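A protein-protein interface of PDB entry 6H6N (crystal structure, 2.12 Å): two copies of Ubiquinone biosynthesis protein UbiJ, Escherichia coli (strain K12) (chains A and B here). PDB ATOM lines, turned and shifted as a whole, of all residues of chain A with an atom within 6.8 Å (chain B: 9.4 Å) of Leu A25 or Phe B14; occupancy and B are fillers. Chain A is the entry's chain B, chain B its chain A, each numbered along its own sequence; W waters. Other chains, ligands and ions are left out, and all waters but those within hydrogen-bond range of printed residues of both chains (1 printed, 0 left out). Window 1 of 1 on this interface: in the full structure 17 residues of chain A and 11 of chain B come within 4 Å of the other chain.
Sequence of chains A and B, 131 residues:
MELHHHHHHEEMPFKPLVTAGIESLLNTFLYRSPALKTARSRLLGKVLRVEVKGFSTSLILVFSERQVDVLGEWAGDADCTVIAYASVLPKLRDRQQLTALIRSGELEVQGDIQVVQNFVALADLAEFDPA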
ATOM      1  N   ALA A  20     -20.388 -34.462  22.777  1.00  0.00           N
ATOM      2  CA  ALA A  20     -19.106 -34.156  23.430  1.00  0.00           C
ATOM      3  C   ALA A  20     -18.206 -33.374  22.457  1.00  0.00           C
ATOM      4  O   ALA A  20     -17.577 -32.394  22.867  1.00  0.00           O
ATOM      5  CB  ALA A  20     -18.404 -35.420  23.891  1.00  0.00           C
ATOM      6  N   GLY A  21     -18.225 -33.768  21.184  1.00  0.00           N
ATOM      7  CA  GLY A  21     -17.485 -33.091  20.128  1.00  0.00           C
ATOM      8  C   GLY A  21     -17.967 -31.675  19.883  1.00  0.00           C
ATOM      9  O   GLY A  21     -17.151 -30.754  19.738  1.00  0.00           O
ATOM     10  N   ILE A  22     -19.303 -31.479  19.842  1.00  0.00           N
ATOM     11  CA  ILE A  22     -19.873 -30.127  19.684  1.00  0.00           C
ATOM     12  C   ILE A  22     -19.551 -29.261  20.924  1.00  0.00           C
ATOM     13  O   ILE A  22     -19.233 -28.087  20.794  1.00  0.00           O
ATOM     14  CB  ILE A  22     -21.386 -30.159  19.315  1.00  0.00           C
ATOM     15  CG1 ILE A  22     -21.569 -30.820  17.908  1.00  0.00           C
ATOM     16  CG2 ILE A  22     -22.003 -28.732  19.360  1.00  0.00           C
ATOM     17  CD1 ILE A  22     -22.931 -31.318  17.583  1.00  0.00           C
ATOM     18  N   GLU A  23     -19.598 -29.855  22.109  1.00  0.00           N
ATOM     19  CA  GLU A  23     -19.295 -29.151  23.349  1.00  0.00           C
ATOM     20  C   GLU A  23     -17.859 -28.595  23.358  1.00  0.00           C
ATOM     21  O   GLU A  23     -17.689 -27.398  23.603  1.00  0.00           O
ATOM     22  CB  GLU A  23     -19.583 -30.022  24.576  1.00  0.00           C
ATOM     23  CG  GLU A  23     -19.315 -29.291  25.871  1.00  0.00           C
ATOM     24  CD  GLU A  23     -19.701 -30.050  27.116  1.00  0.00           C
ATOM     25  OE1 GLU A  23     -20.868 -30.500  27.195  1.00  0.00           O
ATOM     26  OE2 GLU A  23     -18.861 -30.130  28.044  1.00  0.00           O
ATOM     27  N   SER A  24     -16.854 -29.461  23.110  1.00  0.00           N
ATOM     28  CA  SER A  24     -15.441 -29.084  23.044  1.00  0.00           C
ATOM     29  C   SER A  24     -15.197 -27.992  21.960  1.00  0.00           C
ATOM     30  O   SER A  24     -14.421 -27.060  22.195  1.00  0.00           O
ATOM     31  CB  SER A  24     -14.583 -30.314  22.756  1.00  0.00           C
ATOM     32  OG  SER A  24     -13.231 -29.949  22.531  1.00  0.00           O
ATOM     33  N   LEU A  25     -15.850 -28.116  20.786  1.00  0.00           N
ATOM     34  CA  LEU A  25     -15.770 -27.114  19.715  1.00  0.00           C
ATOM     35  C   LEU A  25     -16.279 -25.754  20.213  1.00  0.00           C
ATOM     36  O   LEU A  25     -15.602 -24.755  20.045  1.00  0.00           O
ATOM     37  CB  LEU A  25     -16.605 -27.566  18.501  1.00  0.00           C
ATOM     38  CG  LEU A  25     -16.994 -26.476  17.431  1.00  0.00           C
ATOM     39  CD1 LEU A  25     -15.777 -25.983  16.643  1.00  0.00           C
ATOM     40  CD2 LEU A  25     -18.045 -27.018  16.458  1.00  0.00           C
ATOM     41  N   LEU A  26     -17.481 -25.720  20.811  1.00  0.00           N
ATOM     42  CA  LEU A  26     -18.086 -24.476  21.294  1.00  0.00           C
ATOM     43  C   LEU A  26     -17.308 -23.883  22.456  1.00  0.00           C
ATOM     44  O   LEU A  26     -17.175 -22.672  22.544  1.00  0.00           O
ATOM     45  CB  LEU A  26     -19.544 -24.700  21.678  1.00  0.00           C
ATOM     46  CG  LEU A  26     -20.531 -24.917  20.540  1.00  0.00           C
ATOM     47  CD1 LEU A  26     -21.897 -25.293  21.107  1.00  0.00           C
ATOM     48  CD2 LEU A  26     -20.661 -23.652  19.661  1.00  0.00           C
ATOM     49  N   ASN A  27     -16.748 -24.735  23.322  1.00  0.00           N
ATOM     50  CA  ASN A  27     -15.977 -24.268  24.470  1.00  0.00           C
ATOM     51  C   ASN A  27     -14.624 -23.709  24.069  1.00  0.00           C
ATOM     52  O   ASN A  27     -14.217 -22.699  24.633  1.00  0.00           O
ATOM     53  CB  ASN A  27     -15.877 -25.349  25.557  1.00  0.00           C
ATOM     54  CG  ASN A  27     -17.134 -25.345  26.392  1.00  0.00           C
ATOM     55  OD1 ASN A  27     -17.662 -24.293  26.753  1.00  0.00           O
ATOM     56  ND2 ASN A  27     -17.686 -26.486  26.669  1.00  0.00           N
ATOM     57  N   THR A  28     -13.960 -24.295  23.051  1.00  0.00           N
ATOM     58  CA  THR A  28     -12.675 -23.776  22.568  1.00  0.00           C
ATOM     59  C   THR A  28     -12.902 -22.449  21.849  1.00  0.00           C
ATOM     60  O   THR A  28     -12.146 -21.502  22.053  1.00  0.00           O
ATOM     61  CB  THR A  28     -11.952 -24.797  21.681  1.00  0.00           C
ATOM     62  OG1 THR A  28     -11.903 -26.052  22.362  1.00  0.00           O
ATOM     63  CG2 THR A  28     -10.531 -24.357  21.315  1.00  0.00           C
ATOM     64  N   PHE A  29     -13.957 -22.380  21.034  1.00  0.00           N
ATOM     65  CA  PHE A  29     -14.287 -21.200  20.250  1.00  0.00           C
ATOM     66  C   PHE A  29     -14.815 -20.017  21.067  1.00  0.00           C
ATOM     67  O   PHE A  29     -14.408 -18.899  20.812  1.00  0.00           O
ATOM     68  CB  PHE A  29     -15.279 -21.588  19.126  1.00  0.00           C
ATOM     69  CG  PHE A  29     -15.605 -20.478  18.158  1.00  0.00           C
ATOM     70  CD1 PHE A  29     -14.600 -19.856  17.423  1.00  0.00           C
ATOM     71  CD2 PHE A  29     -16.925 -20.121  17.908  1.00  0.00           C
ATOM     72  CE1 PHE A  29     -14.911 -18.844  16.514  1.00  0.00           C
ATOM     73  CE2 PHE A  29     -17.232 -19.117  16.992  1.00  0.00           C
ATOM     74  CZ  PHE A  29     -16.227 -18.471  16.310  1.00  0.00           C
ATOM     75  N   LEU A  30     -15.730 -20.255  22.022  1.00  0.00           N
ATOM     76  CA  LEU A  30     -16.403 -19.193  22.777  1.00  0.00           C
ATOM     77  C   LEU A  30     -15.932 -18.960  24.190  1.00  0.00           C
ATOM     78  O   LEU A  30     -16.018 -17.821  24.675  1.00  0.00           O
ATOM     79  CB  LEU A  30     -17.931 -19.456  22.805  1.00  0.00           C
ATOM     80  CG  LEU A  30     -18.593 -19.721  21.436  1.00  0.00           C
ATOM     81  CD1 LEU A  30     -19.980 -20.253  21.600  1.00  0.00           C
ATOM     82  CD2 LEU A  30     -18.587 -18.447  20.584  1.00  0.00           C
ATOM     83  N   TYR A  31     -15.461 -20.019  24.864  1.00  0.00           N
ATOM     84  CA  TYR A  31     -15.111 -19.939  26.280  1.00  0.00           C
ATOM     85  C   TYR A  31     -13.622 -19.891  26.622  1.00  0.00           C
ATOM     86  O   TYR A  31     -13.307 -19.664  27.786  1.00  0.00           O
ATOM     87  CB  TYR A  31     -15.776 -21.095  27.040  1.00  0.00           C
ATOM     88  CG  TYR A  31     -17.225 -20.823  27.369  1.00  0.00           C
ATOM     89  CD1 TYR A  31     -18.227 -21.020  26.417  1.00  0.00           C
ATOM     90  CD2 TYR A  31     -17.594 -20.304  28.608  1.00  0.00           C
ATOM     91  CE1 TYR A  31     -19.562 -20.724  26.700  1.00  0.00           C
ATOM     92  CE2 TYR A  31     -18.936 -20.032  28.914  1.00  0.00           C
ATOM     93  CZ  TYR A  31     -19.916 -20.246  27.957  1.00  0.00           C
ATOM     94  OH  TYR A  31     -21.239 -19.995  28.272  1.00  0.00           O
ATOM     95  N   LEU A  89     -26.022 -22.943   9.789  1.00  0.00           N
ATOM     96  CA  LEU A  89     -25.154 -22.918  10.982  1.00  0.00           C
ATOM     97  C   LEU A  89     -23.877 -22.081  10.806  1.00  0.00           C
ATOM     98  O   LEU A  89     -23.650 -21.229  11.673  1.00  0.00           O
ATOM     99  CB  LEU A  89     -24.812 -24.319  11.533  1.00  0.00           C
ATOM    100  CG  LEU A  89     -25.976 -25.117  12.174  1.00  0.00           C
ATOM    101  CD1 LEU A  89     -25.529 -26.516  12.563  1.00  0.00           C
ATOM    102  CD2 LEU A  89     -26.587 -24.404  13.377  1.00  0.00           C
ATOM    103  N   PRO A  90     -23.086 -22.198   9.694  1.00  0.00           N
ATOM    104  CA  PRO A  90     -21.906 -21.321   9.542  1.00  0.00           C
ATOM    105  C   PRO A  90     -22.246 -19.828   9.460  1.00  0.00           C
ATOM    106  O   PRO A  90     -21.394 -18.991   9.784  1.00  0.00           O
ATOM    107  CB  PRO A  90     -21.267 -21.814   8.238  1.00  0.00           C
ATOM    108  CG  PRO A  90     -22.388 -22.434   7.475  1.00  0.00           C
ATOM    109  CD  PRO A  90     -23.191 -23.115   8.536  1.00  0.00           C
ATOM    110  N   ARG A  93     -22.370 -16.707  12.746  1.00  0.00           N
ATOM    111  CA  ARG A  93     -21.171 -16.029  13.268  1.00  0.00           C
ATOM    112  C   ARG A  93     -21.203 -14.551  12.818  1.00  0.00           C
ATOM    113  O   ARG A  93     -20.197 -13.841  12.925  1.00  0.00           O
ATOM    114  CB  ARG A  93     -19.887 -16.718  12.783  1.00  0.00           C
ATOM    115  CG  ARG A  93     -19.612 -18.079  13.409  1.00  0.00           C
ATOM    116  CD  ARG A  93     -18.438 -18.750  12.715  1.00  0.00           C
ATOM    117  NE  ARG A  93     -18.839 -19.474  11.505  1.00  0.00           N
ATOM    118  CZ  ARG A  93     -18.042 -19.715  10.466  1.00  0.00           C
ATOM    119  NH1 ARG A  93     -16.797 -19.253  10.451  1.00  0.00           N
ATOM    120  NH2 ARG A  93     -18.487 -20.408   9.430  1.00  0.00           N
ATOM    121  N   GLU A 127     -14.780 -14.379  16.716  1.00  0.00           N
ATOM    122  CA  GLU A 127     -13.981 -14.611  15.525  1.00  0.00           C
ATOM    123  C   GLU A 127     -13.649 -13.372  14.730  1.00  0.00           C
ATOM    124  O   GLU A 127     -14.504 -12.514  14.527  1.00  0.00           O
ATOM    125  CB  GLU A 127     -14.742 -15.647  14.676  1.00  0.00           C
ATOM    126  CG  GLU A 127     -14.337 -15.842  13.234  1.00  0.00           C
ATOM    127  CD  GLU A 127     -15.413 -16.601  12.483  1.00  0.00           C
ATOM    128  OE1 GLU A 127     -15.229 -17.819  12.262  1.00  0.00           O
ATOM    129  OE2 GLU A 127     -16.481 -16.008  12.209  1.00  0.00           O
ATOM    130  N   GLU B  11      -7.559 -16.267  20.504  1.00  0.00           N
ATOM    131  CA  GLU B  11      -8.685 -16.618  19.620  1.00  0.00           C
ATOM    132  C   GLU B  11      -8.176 -17.347  18.362  1.00  0.00           C
ATOM    133  O   GLU B  11      -7.324 -16.812  17.654  1.00  0.00           O
ATOM    134  CB  GLU B  11      -9.491 -15.362  19.228  1.00  0.00           C
ATOM    135  CG  GLU B  11     -10.420 -14.847  20.320  1.00  0.00           C
ATOM    136  CD  GLU B  11     -10.665 -13.347  20.342  1.00  0.00           C
ATOM    137  OE1 GLU B  11      -9.890 -12.603  19.698  1.00  0.00           O
ATOM    138  OE2 GLU B  11     -11.602 -12.910  21.050  1.00  0.00           O
ATOM    139  N   MET B  12      -8.684 -18.571  18.111  1.00  0.00           N
ATOM    140  CA  MET B  12      -8.288 -19.447  16.994  1.00  0.00           C
ATOM    141  C   MET B  12      -9.426 -19.666  15.967  1.00  0.00           C
ATOM    142  O   MET B  12     -10.582 -19.784  16.375  1.00  0.00           O
ATOM    143  CB  MET B  12      -7.783 -20.795  17.533  1.00  0.00           C
ATOM    144  N   PRO B  13      -9.131 -19.723  14.643  1.00  0.00           N
ATOM    145  CA  PRO B  13     -10.211 -19.865  13.645  1.00  0.00           C
ATOM    146  C   PRO B  13     -11.133 -21.075  13.804  1.00  0.00           C
ATOM    147  O   PRO B  13     -10.737 -22.114  14.338  1.00  0.00           O
ATOM    148  CB  PRO B  13      -9.462 -19.899  12.308  1.00  0.00           C
ATOM    149  CG  PRO B  13      -8.209 -19.173  12.574  1.00  0.00           C
ATOM    150  CD  PRO B  13      -7.825 -19.569  13.975  1.00  0.00           C
ATOM    151  N   PHE B  14     -12.388 -20.901  13.356  1.00  0.00           N
ATOM    152  CA  PHE B  14     -13.461 -21.893  13.435  1.00  0.00           C
ATOM    153  C   PHE B  14     -13.197 -23.143  12.621  1.00  0.00           C
ATOM    154  O   PHE B  14     -13.431 -24.232  13.131  1.00  0.00           O
ATOM    155  CB  PHE B  14     -14.811 -21.257  13.040  1.00  0.00           C
ATOM    156  CG  PHE B  14     -16.039 -22.096  13.291  1.00  0.00           C
ATOM    157  CD1 PHE B  14     -16.463 -22.368  14.588  1.00  0.00           C
ATOM    158  CD2 PHE B  14     -16.807 -22.563  12.233  1.00  0.00           C
ATOM    159  CE1 PHE B  14     -17.621 -23.120  14.823  1.00  0.00           C
ATOM    160  CE2 PHE B  14     -17.971 -23.299  12.465  1.00  0.00           C
ATOM    161  CZ  PHE B  14     -18.364 -23.586  13.759  1.00  0.00           C
ATOM    162  N   LYS B  15     -12.747 -22.994  11.358  1.00  0.00           N
ATOM    163  CA  LYS B  15     -12.465 -24.080  10.403  1.00  0.00           C
ATOM    164  C   LYS B  15     -11.495 -25.182  10.978  1.00  0.00           C
ATOM    165  O   LYS B  15     -11.931 -26.316  11.061  1.00  0.00           O
ATOM    166  CB  LYS B  15     -11.960 -23.463   9.062  1.00  0.00           C
ATOM    167  CG  LYS B  15     -11.443 -24.443   8.014  1.00  0.00           C
ATOM    168  CD  LYS B  15     -12.545 -25.229   7.312  1.00  0.00           C
ATOM    169  CE  LYS B  15     -11.933 -26.225   6.357  1.00  0.00           C
ATOM    170  NZ  LYS B  15     -12.939 -27.175   5.829  1.00  0.00           N
ATOM    171  N   PRO B  16     -10.239 -24.874  11.437  1.00  0.00           N
ATOM    172  CA  PRO B  16      -9.379 -25.916  12.050  1.00  0.00           C
ATOM    173  C   PRO B  16      -9.991 -26.577  13.309  1.00  0.00           C
ATOM    174  O   PRO B  16      -9.668 -27.714  13.607  1.00  0.00           O
ATOM    175  CB  PRO B  16      -8.092 -25.154  12.383  1.00  0.00           C
ATOM    176  CG  PRO B  16      -8.120 -23.942  11.465  1.00  0.00           C
ATOM    177  CD  PRO B  16      -9.561 -23.559  11.471  1.00  0.00           C
ATOM    178  N   LEU B  17     -10.913 -25.892  14.002  1.00  0.00           N
ATOM    179  CA  LEU B  17     -11.617 -26.449  15.156  1.00  0.00           C
ATOM    180  C   LEU B  17     -12.673 -27.475  14.707  1.00  0.00           C
ATOM    181  O   LEU B  17     -12.827 -28.497  15.377  1.00  0.00           O
ATOM    182  CB  LEU B  17     -12.253 -25.333  16.023  1.00  0.00           C
ATOM    183  CG  LEU B  17     -11.320 -24.442  16.817  1.00  0.00           C
ATOM    184  CD1 LEU B  17     -12.108 -23.465  17.675  1.00  0.00           C
ATOM    185  CD2 LEU B  17     -10.381 -25.256  17.691  1.00  0.00           C
ATOM    186  N   VAL B  18     -13.361 -27.225  13.558  1.00  0.00           N
ATOM    187  CA  VAL B  18     -14.327 -28.143  12.948  1.00  0.00           C
ATOM    188  C   VAL B  18     -13.617 -29.431  12.485  1.00  0.00           C
ATOM    189  O   VAL B  18     -14.091 -30.500  12.827  1.00  0.00           O
ATOM    190  CB  VAL B  18     -15.147 -27.499  11.799  1.00  0.00           C
ATOM    191  CG1 VAL B  18     -16.084 -28.517  11.152  1.00  0.00           C
ATOM    192  CG2 VAL B  18     -15.949 -26.316  12.306  1.00  0.00           C
ATOM    193  N   THR B  19     -12.500 -29.329  11.728  1.00  0.00           N
ATOM    194  CA  THR B  19     -11.754 -30.494  11.236  1.00  0.00           C
ATOM    195  C   THR B  19     -11.136 -31.281  12.365  1.00  0.00           C
ATOM    196  O   THR B  19     -11.153 -32.506  12.289  1.00  0.00           O
ATOM    197  CB  THR B  19     -10.709 -30.164  10.132  1.00  0.00           C
ATOM    198  OG1 THR B  19      -9.693 -29.349  10.678  1.00  0.00           O
ATOM    199  CG2 THR B  19     -11.309 -29.492   8.933  1.00  0.00           C
ATOM    200  N   ALA B  20     -10.602 -30.598  13.415  1.00  0.00           N
ATOM    201  CA  ALA B  20     -10.022 -31.289  14.577  1.00  0.00           C
ATOM    202  C   ALA B  20     -11.128 -32.076  15.299  1.00  0.00           C
ATOM    203  O   ALA B  20     -10.907 -33.239  15.661  1.00  0.00           O
ATOM    204  CB  ALA B  20      -9.371 -30.290  15.526  1.00  0.00           C
ATOM    205  N   GLY B  21     -12.309 -31.448  15.453  1.00  0.00           N
ATOM    206  CA  GLY B  21     -13.491 -32.059  16.058  1.00  0.00           C
ATOM    207  C   GLY B  21     -14.001 -33.257  15.277  1.00  0.00           C
ATOM    208  O   GLY B  21     -14.303 -34.296  15.875  1.00  0.00           O
ATOM    209  N   ILE B  22     -14.058 -33.147  13.933  1.00  0.00           N
ATOM    210  CA  ILE B  22     -14.477 -34.277  13.078  1.00  0.00           C
ATOM    211  C   ILE B  22     -13.445 -35.412  13.176  1.00  0.00           C
ATOM    212  O   ILE B  22     -13.819 -36.576  13.251  1.00  0.00           O
ATOM    213  CB  ILE B  22     -14.817 -33.836  11.613  1.00  0.00           C
ATOM    214  CG1 ILE B  22     -16.057 -32.929  11.600  1.00  0.00           C
ATOM    215  CG2 ILE B  22     -15.038 -35.039  10.686  1.00  0.00           C
ATOM    216  CD1 ILE B  22     -16.235 -32.082  10.319  1.00  0.00           C
ATOM    217  N   SER B  24     -11.359 -36.176  15.754  1.00  0.00           N
ATOM    218  CA  SER B  24     -11.500 -36.774  17.081  1.00  0.00           C
ATOM    219  C   SER B  24     -12.669 -37.753  17.098  1.00  0.00           C
ATOM    220  O   SER B  24     -12.487 -38.902  17.501  1.00  0.00           O
ATOM    221  CB  SER B  24     -11.676 -35.682  18.130  1.00  0.00           C
ATOM    222  OG  SER B  24     -11.726 -36.289  19.407  1.00  0.00           O
ATOM    223  N   PHE B  55     -21.832 -25.388   2.075  1.00  0.00           N
ATOM    224  CA  PHE B  55     -20.617 -25.002   2.794  1.00  0.00           C
ATOM    225  C   PHE B  55     -19.537 -24.632   1.762  1.00  0.00           C
ATOM    226  O   PHE B  55     -19.479 -25.213   0.670  1.00  0.00           O
ATOM    227  CB  PHE B  55     -20.146 -26.146   3.711  1.00  0.00           C
ATOM    228  CG  PHE B  55     -21.033 -26.401   4.906  1.00  0.00           C
ATOM    229  CD1 PHE B  55     -22.161 -27.212   4.799  1.00  0.00           C
ATOM    230  CD2 PHE B  55     -20.740 -25.837   6.140  1.00  0.00           C
ATOM    231  CE1 PHE B  55     -22.988 -27.447   5.905  1.00  0.00           C
ATOM    232  CE2 PHE B  55     -21.552 -26.092   7.253  1.00  0.00           C
ATOM    233  CZ  PHE B  55     -22.668 -26.900   7.128  1.00  0.00           C
ATOM    234  N   THR B  57     -16.110 -24.801   2.177  1.00  0.00           N
ATOM    235  CA  THR B  57     -14.888 -25.597   2.270  1.00  0.00           C
ATOM    236  C   THR B  57     -15.104 -27.128   2.278  1.00  0.00           C
ATOM    237  O   THR B  57     -16.062 -27.625   2.860  1.00  0.00           O
ATOM    238  CB  THR B  57     -14.073 -25.156   3.497  1.00  0.00           C
ATOM    239  OG1 THR B  57     -14.823 -25.428   4.683  1.00  0.00           O
ATOM    240  CG2 THR B  57     -13.661 -23.680   3.453  1.00  0.00           C
ATOM    241  N   LEU B  59     -13.794 -31.249   3.085  1.00  0.00           N
ATOM    242  CA  LEU B  59     -13.248 -32.059   4.163  1.00  0.00           C
ATOM    243  C   LEU B  59     -12.479 -33.187   3.487  1.00  0.00           C
ATOM    244  O   LEU B  59     -13.009 -33.844   2.583  1.00  0.00           O
ATOM    245  CB  LEU B  59     -14.334 -32.663   5.080  1.00  0.00           C
ATOM    246  CG  LEU B  59     -15.206 -31.736   5.925  1.00  0.00           C
ATOM    247  CD1 LEU B  59     -16.362 -32.547   6.551  1.00  0.00           C
ATOM    248  CD2 LEU B  59     -14.413 -31.094   7.047  1.00  0.00           C
HETATM  249  O   HOH W   1     -12.639 -18.237  11.901  1.00  0.00           O
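Water W1 lies within hydrogen-bond range of the side-chain carboxylate (OE1) of Glu A127 and the backbone NH (N) of Phe B14.
Among the printed residues, merely in contact across the chains: Glu A127 with Phe B14, Arg A93 with Phe B14, Pro A90 with Phe B55, Leu A25 with Leu B17, Thr A28 with Leu B17, Leu A25 with Phe B14 and Phe A29 with Leu B17.
Printed residues of chain B within 4 Å of Leu A25: Phe B14 (3.9 Å) and Leu B17 (3.6 Å).
Of the printed residues of chain B, Phe A29 touches Leu B17.
Of the printed residues of chain B, Pro A90 touches Phe B55 (3.6 Å).
Of the printed residues of chain B, Arg A93 touches Phe B14 (3.6 Å).
Of the printed residues of chain B, Glu A127 touches Phe B14.
Phe B14 touches just these residues of chain A: Leu A25 (3.9 Å), Arg A93 (3.6 Å) and Glu A127 (3.5 Å).
Printed residues of chain A within 4 Å of Leu B17: Leu A25 (3.6 Å), Thr A28 (3.7 Å) and Phe A29 (3.96 Å).
Thr B19 touches none of the printed residues of chain A.
Of the 16 printed residues of chain A, 6 touch a printed residue of chain B.
Hydrophobic or aromatic side chains of chain B that line the printed part of chain A: Phe B14, Leu B17 and Phe B55.
Among the printed residues, 7 pairs touch across the chains.
Among the printed residues, no Asp or Glu carboxylate lies within 4 Å of a Lys or Arg side-chain nitrogen of the other chain.
Positions printed for both chains: 20, 21, 22 and 24.
The backbone carbonyl oxygen of Ser A24 sits at hydrogen-bond distance from the side-chain hydroxyl of Thr A28 (2.7 Å).
O of Pro A90 lies within hydrogen-bond range of NE of Arg A93 (3.1 Å).
The side-chain carboxylate (OE1) of Glu A127 lies within salt-bridge range of the guanidinium group (NH1) of Arg A93 (2.8 Å).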
